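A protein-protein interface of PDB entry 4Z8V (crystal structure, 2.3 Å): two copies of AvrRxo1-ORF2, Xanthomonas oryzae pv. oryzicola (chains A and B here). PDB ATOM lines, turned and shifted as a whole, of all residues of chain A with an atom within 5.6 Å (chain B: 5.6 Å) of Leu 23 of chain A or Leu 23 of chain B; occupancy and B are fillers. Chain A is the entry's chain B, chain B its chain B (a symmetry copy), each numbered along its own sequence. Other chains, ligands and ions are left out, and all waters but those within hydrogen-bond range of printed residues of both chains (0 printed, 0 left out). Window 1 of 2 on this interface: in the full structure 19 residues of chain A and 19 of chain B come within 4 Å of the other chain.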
ATOM      1  N   GLU A  18     -30.969   9.076  21.066  1.00  0.00           N
ATOM      2  CA  GLU A  18     -31.473   7.760  21.440  1.00  0.00           C
ATOM      3  C   GLU A  18     -30.610   7.200  22.545  1.00  0.00           C
ATOM      4  O   GLU A  18     -31.109   6.556  23.461  1.00  0.00           O
ATOM      5  CB  GLU A  18     -31.458   6.805  20.239  1.00  0.00           C
ATOM      6  CG  GLU A  18     -32.254   7.335  19.052  1.00  0.00           C
ATOM      7  CD  GLU A  18     -32.214   6.404  17.861  1.00  0.00           C
ATOM      8  OE1 GLU A  18     -31.677   5.279  18.004  1.00  0.00           O
ATOM      9  OE2 GLU A  18     -32.727   6.805  16.788  1.00  0.00           O
ATOM     10  N   ARG A  19     -29.307   7.431  22.444  1.00  0.00           N
ATOM     11  CA  ARG A  19     -28.394   6.881  23.422  1.00  0.00           C
ATOM     12  C   ARG A  19     -28.731   7.499  24.766  1.00  0.00           C
ATOM     13  O   ARG A  19     -28.916   6.775  25.755  1.00  0.00           O
ATOM     14  CB  ARG A  19     -26.957   7.197  23.037  1.00  0.00           C
ATOM     15  CG  ARG A  19     -25.941   6.798  24.072  1.00  0.00           C
ATOM     16  CD  ARG A  19     -24.605   7.476  23.772  1.00  0.00           C
ATOM     17  NE  ARG A  19     -23.567   7.094  24.722  1.00  0.00           N
ATOM     18  CZ  ARG A  19     -22.760   6.047  24.560  1.00  0.00           C
ATOM     19  NH1 ARG A  19     -22.880   5.264  23.486  1.00  0.00           N
ATOM     20  NH2 ARG A  19     -21.831   5.777  25.471  1.00  0.00           N
ATOM     21  N   ASN A  20     -28.857   8.828  24.800  1.00  0.00           N
ATOM     22  CA  ASN A  20     -29.127   9.507  26.063  1.00  0.00           C
ATOM     23  C   ASN A  20     -30.515   9.212  26.632  1.00  0.00           C
ATOM     24  O   ASN A  20     -30.699   9.225  27.845  1.00  0.00           O
ATOM     25  CB  ASN A  20     -28.890  11.014  25.932  1.00  0.00           C
ATOM     26  CG  ASN A  20     -27.437  11.343  25.656  1.00  0.00           C
ATOM     27  OD1 ASN A  20     -26.529  10.593  26.050  1.00  0.00           O
ATOM     28  ND2 ASN A  20     -27.202  12.453  24.949  1.00  0.00           N
ATOM     29  N   LYS A  21     -31.484   8.932  25.761  1.00  0.00           N
ATOM     30  CA  LYS A  21     -32.824   8.552  26.216  1.00  0.00           C
ATOM     31  C   LYS A  21     -32.833   7.161  26.881  1.00  0.00           C
ATOM     32  O   LYS A  21     -33.484   6.962  27.908  1.00  0.00           O
ATOM     33  CB  LYS A  21     -33.829   8.625  25.060  1.00  0.00           C
ATOM     34  CG  LYS A  21     -35.190   8.021  25.388  1.00  0.00           C
ATOM     35  CD  LYS A  21     -36.236   8.264  24.298  1.00  0.00           C
ATOM     36  CE  LYS A  21     -36.745   9.715  24.324  1.00  0.00           C
ATOM     37  NZ  LYS A  21     -37.936   9.955  23.440  1.00  0.00           N
ATOM     38  N   ALA A  22     -32.090   6.210  26.319  1.00  0.00           N
ATOM     39  CA  ALA A  22     -31.955   4.888  26.945  1.00  0.00           C
ATOM     40  C   ALA A  22     -31.217   5.006  28.280  1.00  0.00           C
ATOM     41  O   ALA A  22     -31.630   4.410  29.279  1.00  0.00           O
ATOM     42  CB  ALA A  22     -31.244   3.913  26.017  1.00  0.00           C
ATOM     43  N   LEU A  23     -30.132   5.784  28.299  1.00  0.00           N
ATOM     44  CA  LEU A  23     -29.422   6.082  29.544  1.00  0.00           C
ATOM     45  C   LEU A  23     -30.347   6.746  30.554  1.00  0.00           C
ATOM     46  O   LEU A  23     -30.393   6.348  31.723  1.00  0.00           O
ATOM     47  CB  LEU A  23     -28.224   6.977  29.268  1.00  0.00           C
ATOM     48  CG  LEU A  23     -27.154   6.256  28.454  1.00  0.00           C
ATOM     49  CD1 LEU A  23     -26.005   7.190  28.093  1.00  0.00           C
ATOM     50  CD2 LEU A  23     -26.640   5.050  29.247  1.00  0.00           C
ATOM     51  N   HIS A  24     -31.094   7.748  30.098  1.00  0.00           N
ATOM     52  CA  HIS A  24     -32.043   8.446  30.960  1.00  0.00           C
ATOM     53  C   HIS A  24     -33.005   7.444  31.598  1.00  0.00           C
ATOM     54  O   HIS A  24     -33.151   7.390  32.826  1.00  0.00           O
ATOM     55  CB  HIS A  24     -32.839   9.454  30.143  1.00  0.00           C
ATOM     56  CG  HIS A  24     -33.558  10.473  30.961  1.00  0.00           C
ATOM     57  ND1 HIS A  24     -32.917  11.277  31.885  1.00  0.00           N
ATOM     58  CD2 HIS A  24     -34.862  10.847  30.979  1.00  0.00           C
ATOM     59  CE1 HIS A  24     -33.798  12.091  32.438  1.00  0.00           C
ATOM     60  NE2 HIS A  24     -34.983  11.851  31.908  1.00  0.00           N
ATOM     61  N   ALA A  25     -33.656   6.643  30.758  1.00  0.00           N
ATOM     62  CA  ALA A  25     -34.625   5.668  31.255  1.00  0.00           C
ATOM     63  C   ALA A  25     -33.946   4.688  32.211  1.00  0.00           C
ATOM     64  O   ALA A  25     -34.430   4.431  33.315  1.00  0.00           O
ATOM     65  CB  ALA A  25     -35.288   4.915  30.083  1.00  0.00           C
ATOM     66  N   SER A  26     -32.822   4.146  31.766  1.00  0.00           N
ATOM     67  CA  SER A  26     -32.094   3.125  32.506  1.00  0.00           C
ATOM     68  C   SER A  26     -31.604   3.597  33.896  1.00  0.00           C
ATOM     69  O   SER A  26     -31.631   2.830  34.872  1.00  0.00           O
ATOM     70  CB  SER A  26     -30.922   2.637  31.646  1.00  0.00           C
ATOM     71  OG  SER A  26     -29.928   2.034  32.435  1.00  0.00           O
ATOM     72  N   ASP A  27     -31.172   4.847  34.000  1.00  0.00           N
ATOM     73  CA  ASP A  27     -30.744   5.380  35.295  1.00  0.00           C
ATOM     74  C   ASP A  27     -31.852   5.293  36.346  1.00  0.00           C
ATOM     75  O   ASP A  27     -31.607   4.908  37.497  1.00  0.00           O
ATOM     76  CB  ASP A  27     -30.312   6.841  35.158  1.00  0.00           C
ATOM     77  CG  ASP A  27     -28.921   6.995  34.569  1.00  0.00           C
ATOM     78  OD1 ASP A  27     -28.141   6.019  34.604  1.00  0.00           O
ATOM     79  OD2 ASP A  27     -28.606   8.114  34.098  1.00  0.00           O
ATOM     80  N   LEU A  28     -33.064   5.673  35.959  1.00  0.00           N
ATOM     81  CA  LEU A  28     -34.201   5.606  36.878  1.00  0.00           C
ATOM     82  C   LEU A  28     -34.577   4.165  37.188  1.00  0.00           C
ATOM     83  O   LEU A  28     -34.810   3.817  38.351  1.00  0.00           O
ATOM     84  CB  LEU A  28     -35.418   6.332  36.297  1.00  0.00           C
ATOM     85  CG  LEU A  28     -36.713   6.215  37.112  1.00  0.00           C
ATOM     86  CD1 LEU A  28     -36.533   6.761  38.525  1.00  0.00           C
ATOM     87  CD2 LEU A  28     -37.855   6.943  36.398  1.00  0.00           C
ATOM     88  N   GLU B  18     -30.232  -4.447  29.384  1.00  0.00           N
ATOM     89  CA  GLU B  18     -30.841  -3.576  28.385  1.00  0.00           C
ATOM     90  C   GLU B  18     -29.996  -2.333  28.241  1.00  0.00           C
ATOM     91  O   GLU B  18     -29.824  -1.819  27.141  1.00  0.00           O
ATOM     92  CB  GLU B  18     -32.268  -3.187  28.792  1.00  0.00           C
ATOM     93  CG  GLU B  18     -33.167  -4.396  29.025  1.00  0.00           C
ATOM     94  CD  GLU B  18     -34.565  -4.009  29.452  1.00  0.00           C
ATOM     95  OE1 GLU B  18     -34.876  -2.793  29.436  1.00  0.00           O
ATOM     96  OE2 GLU B  18     -35.346  -4.928  29.796  1.00  0.00           O
ATOM     97  N   ARG B  19     -29.487  -1.837  29.361  1.00  0.00           N
ATOM     98  CA  ARG B  19     -28.716  -0.614  29.330  1.00  0.00           C
ATOM     99  C   ARG B  19     -27.477  -0.870  28.494  1.00  0.00           C
ATOM    100  O   ARG B  19     -27.181  -0.102  27.568  1.00  0.00           O
ATOM    101  CB  ARG B  19     -28.330  -0.199  30.741  1.00  0.00           C
ATOM    102  CG  ARG B  19     -27.398   0.980  30.803  1.00  0.00           C
ATOM    103  CD  ARG B  19     -26.785   1.083  32.199  1.00  0.00           C
ATOM    104  NE  ARG B  19     -25.901   2.234  32.330  1.00  0.00           N
ATOM    105  CZ  ARG B  19     -26.306   3.442  32.718  1.00  0.00           C
ATOM    106  NH1 ARG B  19     -27.592   3.662  33.002  1.00  0.00           N
ATOM    107  NH2 ARG B  19     -25.430   4.436  32.823  1.00  0.00           N
ATOM    108  N   ASN B  20     -26.774  -1.968  28.785  1.00  0.00           N
ATOM    109  CA  ASN B  20     -25.539  -2.261  28.065  1.00  0.00           C
ATOM    110  C   ASN B  20     -25.758  -2.609  26.592  1.00  0.00           C
ATOM    111  O   ASN B  20     -24.892  -2.349  25.762  1.00  0.00           O
ATOM    112  CB  ASN B  20     -24.738  -3.352  28.780  1.00  0.00           C
ATOM    113  CG  ASN B  20     -24.256  -2.905  30.145  1.00  0.00           C
ATOM    114  OD1 ASN B  20     -24.041  -1.706  30.382  1.00  0.00           O
ATOM    115  ND2 ASN B  20     -24.109  -3.862  31.066  1.00  0.00           N
ATOM    116  N   LYS B  21     -26.916  -3.181  26.266  1.00  0.00           N
ATOM    117  CA  LYS B  21     -27.250  -3.471  24.869  1.00  0.00           C
ATOM    118  C   LYS B  21     -27.501  -2.185  24.058  1.00  0.00           C
ATOM    119  O   LYS B  21     -27.058  -2.068  22.914  1.00  0.00           O
ATOM    120  CB  LYS B  21     -28.447  -4.427  24.786  1.00  0.00           C
ATOM    121  CG  LYS B  21     -29.006  -4.592  23.377  1.00  0.00           C
ATOM    122  CD  LYS B  21     -30.075  -5.682  23.278  1.00  0.00           C
ATOM    123  CE  LYS B  21     -29.449  -7.086  23.317  1.00  0.00           C
ATOM    124  NZ  LYS B  21     -30.415  -8.189  22.989  1.00  0.00           N
ATOM    125  N   ALA B  22     -28.182  -1.208  24.655  1.00  0.00           N
ATOM    126  CA  ALA B  22     -28.374   0.090  23.997  1.00  0.00           C
ATOM    127  C   ALA B  22     -27.032   0.806  23.832  1.00  0.00           C
ATOM    128  O   ALA B  22     -26.740   1.352  22.764  1.00  0.00           O
ATOM    129  CB  ALA B  22     -29.358   0.956  24.770  1.00  0.00           C
ATOM    130  N   LEU B  23     -26.211   0.791  24.885  1.00  0.00           N
ATOM    131  CA  LEU B  23     -24.850   1.323  24.806  1.00  0.00           C
ATOM    132  C   LEU B  23     -24.048   0.610  23.726  1.00  0.00           C
ATOM    133  O   LEU B  23     -23.388   1.253  22.902  1.00  0.00           O
ATOM    134  CB  LEU B  23     -24.150   1.187  26.150  1.00  0.00           C
ATOM    135  CG  LEU B  23     -24.783   2.084  27.210  1.00  0.00           C
ATOM    136  CD1 LEU B  23     -24.144   1.866  28.576  1.00  0.00           C
ATOM    137  CD2 LEU B  23     -24.651   3.548  26.780  1.00  0.00           C
ATOM    138  N   HIS B  24     -24.116  -0.719  23.724  1.00  0.00           N
ATOM    139  CA  HIS B  24     -23.417  -1.517  22.721  1.00  0.00           C
ATOM    140  C   HIS B  24     -23.815  -1.060  21.318  1.00  0.00           C
ATOM    141  O   HIS B  24     -22.960  -0.722  20.489  1.00  0.00           O
ATOM    142  CB  HIS B  24     -23.775  -2.987  22.890  1.00  0.00           C
ATOM    143  CG  HIS B  24     -22.853  -3.925  22.185  1.00  0.00           C
ATOM    144  ND1 HIS B  24     -21.486  -3.925  22.391  1.00  0.00           N
ATOM    145  CD2 HIS B  24     -23.098  -4.920  21.296  1.00  0.00           C
ATOM    146  CE1 HIS B  24     -20.935  -4.871  21.651  1.00  0.00           C
ATOM    147  NE2 HIS B  24     -21.889  -5.488  20.979  1.00  0.00           N
ATOM    148  N   ALA B  25     -25.120  -1.043  21.057  1.00  0.00           N
ATOM    149  CA  ALA B  25     -25.613  -0.654  19.738  1.00  0.00           C
ATOM    150  C   ALA B  25     -25.176   0.774  19.409  1.00  0.00           C
ATOM    151  O   ALA B  25     -24.645   1.049  18.332  1.00  0.00           O
ATOM    152  CB  ALA B  25     -27.149  -0.781  19.673  1.00  0.00           C
ATOM    153  N   SER B  26     -25.411   1.672  20.355  1.00  0.00           N
ATOM    154  CA  SER B  26     -25.143   3.091  20.175  1.00  0.00           C
ATOM    155  C   SER B  26     -23.655   3.413  19.898  1.00  0.00           C
ATOM    156  O   SER B  26     -23.337   4.296  19.086  1.00  0.00           O
ATOM    157  CB  SER B  26     -25.647   3.847  21.411  1.00  0.00           C
ATOM    158  OG  SER B  26     -25.021   5.099  21.533  1.00  0.00           O
ATOM    159  N   ASP B  27     -22.744   2.700  20.549  1.00  0.00           N
ATOM    160  CA  ASP B  27     -21.317   2.910  20.298  1.00  0.00           C
ATOM    161  C   ASP B  27     -20.956   2.697  18.827  1.00  0.00           C
ATOM    162  O   ASP B  27     -20.201   3.484  18.238  1.00  0.00           O
ATOM    163  CB  ASP B  27     -20.476   1.959  21.152  1.00  0.00           C
ATOM    164  CG  ASP B  27     -20.349   2.412  22.595  1.00  0.00           C
ATOM    165  OD1 ASP B  27     -20.576   3.611  22.871  1.00  0.00           O
ATOM    166  OD2 ASP B  27     -19.989   1.564  23.445  1.00  0.00           O
ATOM    167  N   LEU B  28     -21.474   1.625  18.241  1.00  0.00           N
ATOM    168  CA  LEU B  28     -21.212   1.341  16.829  1.00  0.00           C
ATOM    169  C   LEU B  28     -21.891   2.360  15.926  1.00  0.00           C
ATOM    170  O   LEU B  28     -21.277   2.861  14.978  1.00  0.00           O
ATOM    171  CB  LEU B  28     -21.692  -0.064  16.455  1.00  0.00           C
ATOM    172  CG  LEU B  28     -21.594  -0.426  14.967  1.00  0.00           C
ATOM    173  CD1 LEU B  28     -20.157  -0.326  14.464  1.00  0.00           C
ATOM    174  CD2 LEU B  28     -22.147  -1.833  14.727  1.00  0.00           C
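OG of Ser 26 of chain B lies within hydrogen-bond range of NH1 of Arg 19 of chain A (2.9 Å). NH1 of Arg 19 of chain A lies within salt-bridge range of OD1 of Asp 27 of chain B, at 2.9 Å. The side-chain hydroxyl (OG) of Ser 26 of chain A is in hydrogen-bond range of the guanidinium group (NH1) of Arg 19 of chain B (2.9 Å). OD1 of Asp 27 of chain A lies within salt-bridge range of NH1 of Arg 19 of chain B, 2.9 Å away.
Among the printed residues, merely in contact across the chains: Arg 19 of chain A with Leu 23 of chain B, Ala 22 of chain A with Ala 22 of chain B, Leu 23 of chain A with Arg 19 of chain B and Leu 23 of chain A with Leu 23 of chain B.
Leu 23 of chain A touches two residues of chain B. Of chain A, only Arg 19 (3.8 Å) and Leu 23 (3.5 Å) come within 4 Å of Leu 23 of chain B. Of the printed residues of chain A, Arg 19 of chain B touches Leu 23, Ser 26 and Asp 27. Of the printed residues of chain A, Ala 22 of chain B touches Ala 22 (3.7 Å). Of the printed residues of chain B, Ala 22 of chain A touches Ala 22. Of the printed residues of chain B, Ser 26 of chain A touches Arg 19 (2.9 Å). Printed residues of chain B within 4 Å of Asp 27 of chain A: Arg 19 (2.9 Å).
Printed residues of chain A that touch a printed residue of chain B: Arg 19, Ala 22, Leu 23, Ser 26 and Asp 27. Hydrophobic or aromatic side chains of chain B that line the printed part of chain A: Ala 22 and Leu 23. Among the printed residues, 8 pairs touch across the chains.
Arg 19 of chain A touches Leu 23 of chain B, and with the chains exchanged Leu 23 of chain A touches Arg 19 of chain B. Arg 19 of chain A touches Ser 26 of chain B, and with the chains exchanged Ser 26 of chain A touches Arg 19 of chain B. Arg 19 of chain A touches Asp 27 of chain B, and with the chains exchanged Asp 27 of chain A touches Arg 19 of chain B. Ala 22 of chain B touches its own counterpart, Ala 22 of chain A. Of the 8 pairs that touch across the chains among the printed residues, 8 have their exchanged pair printed and touching as well.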
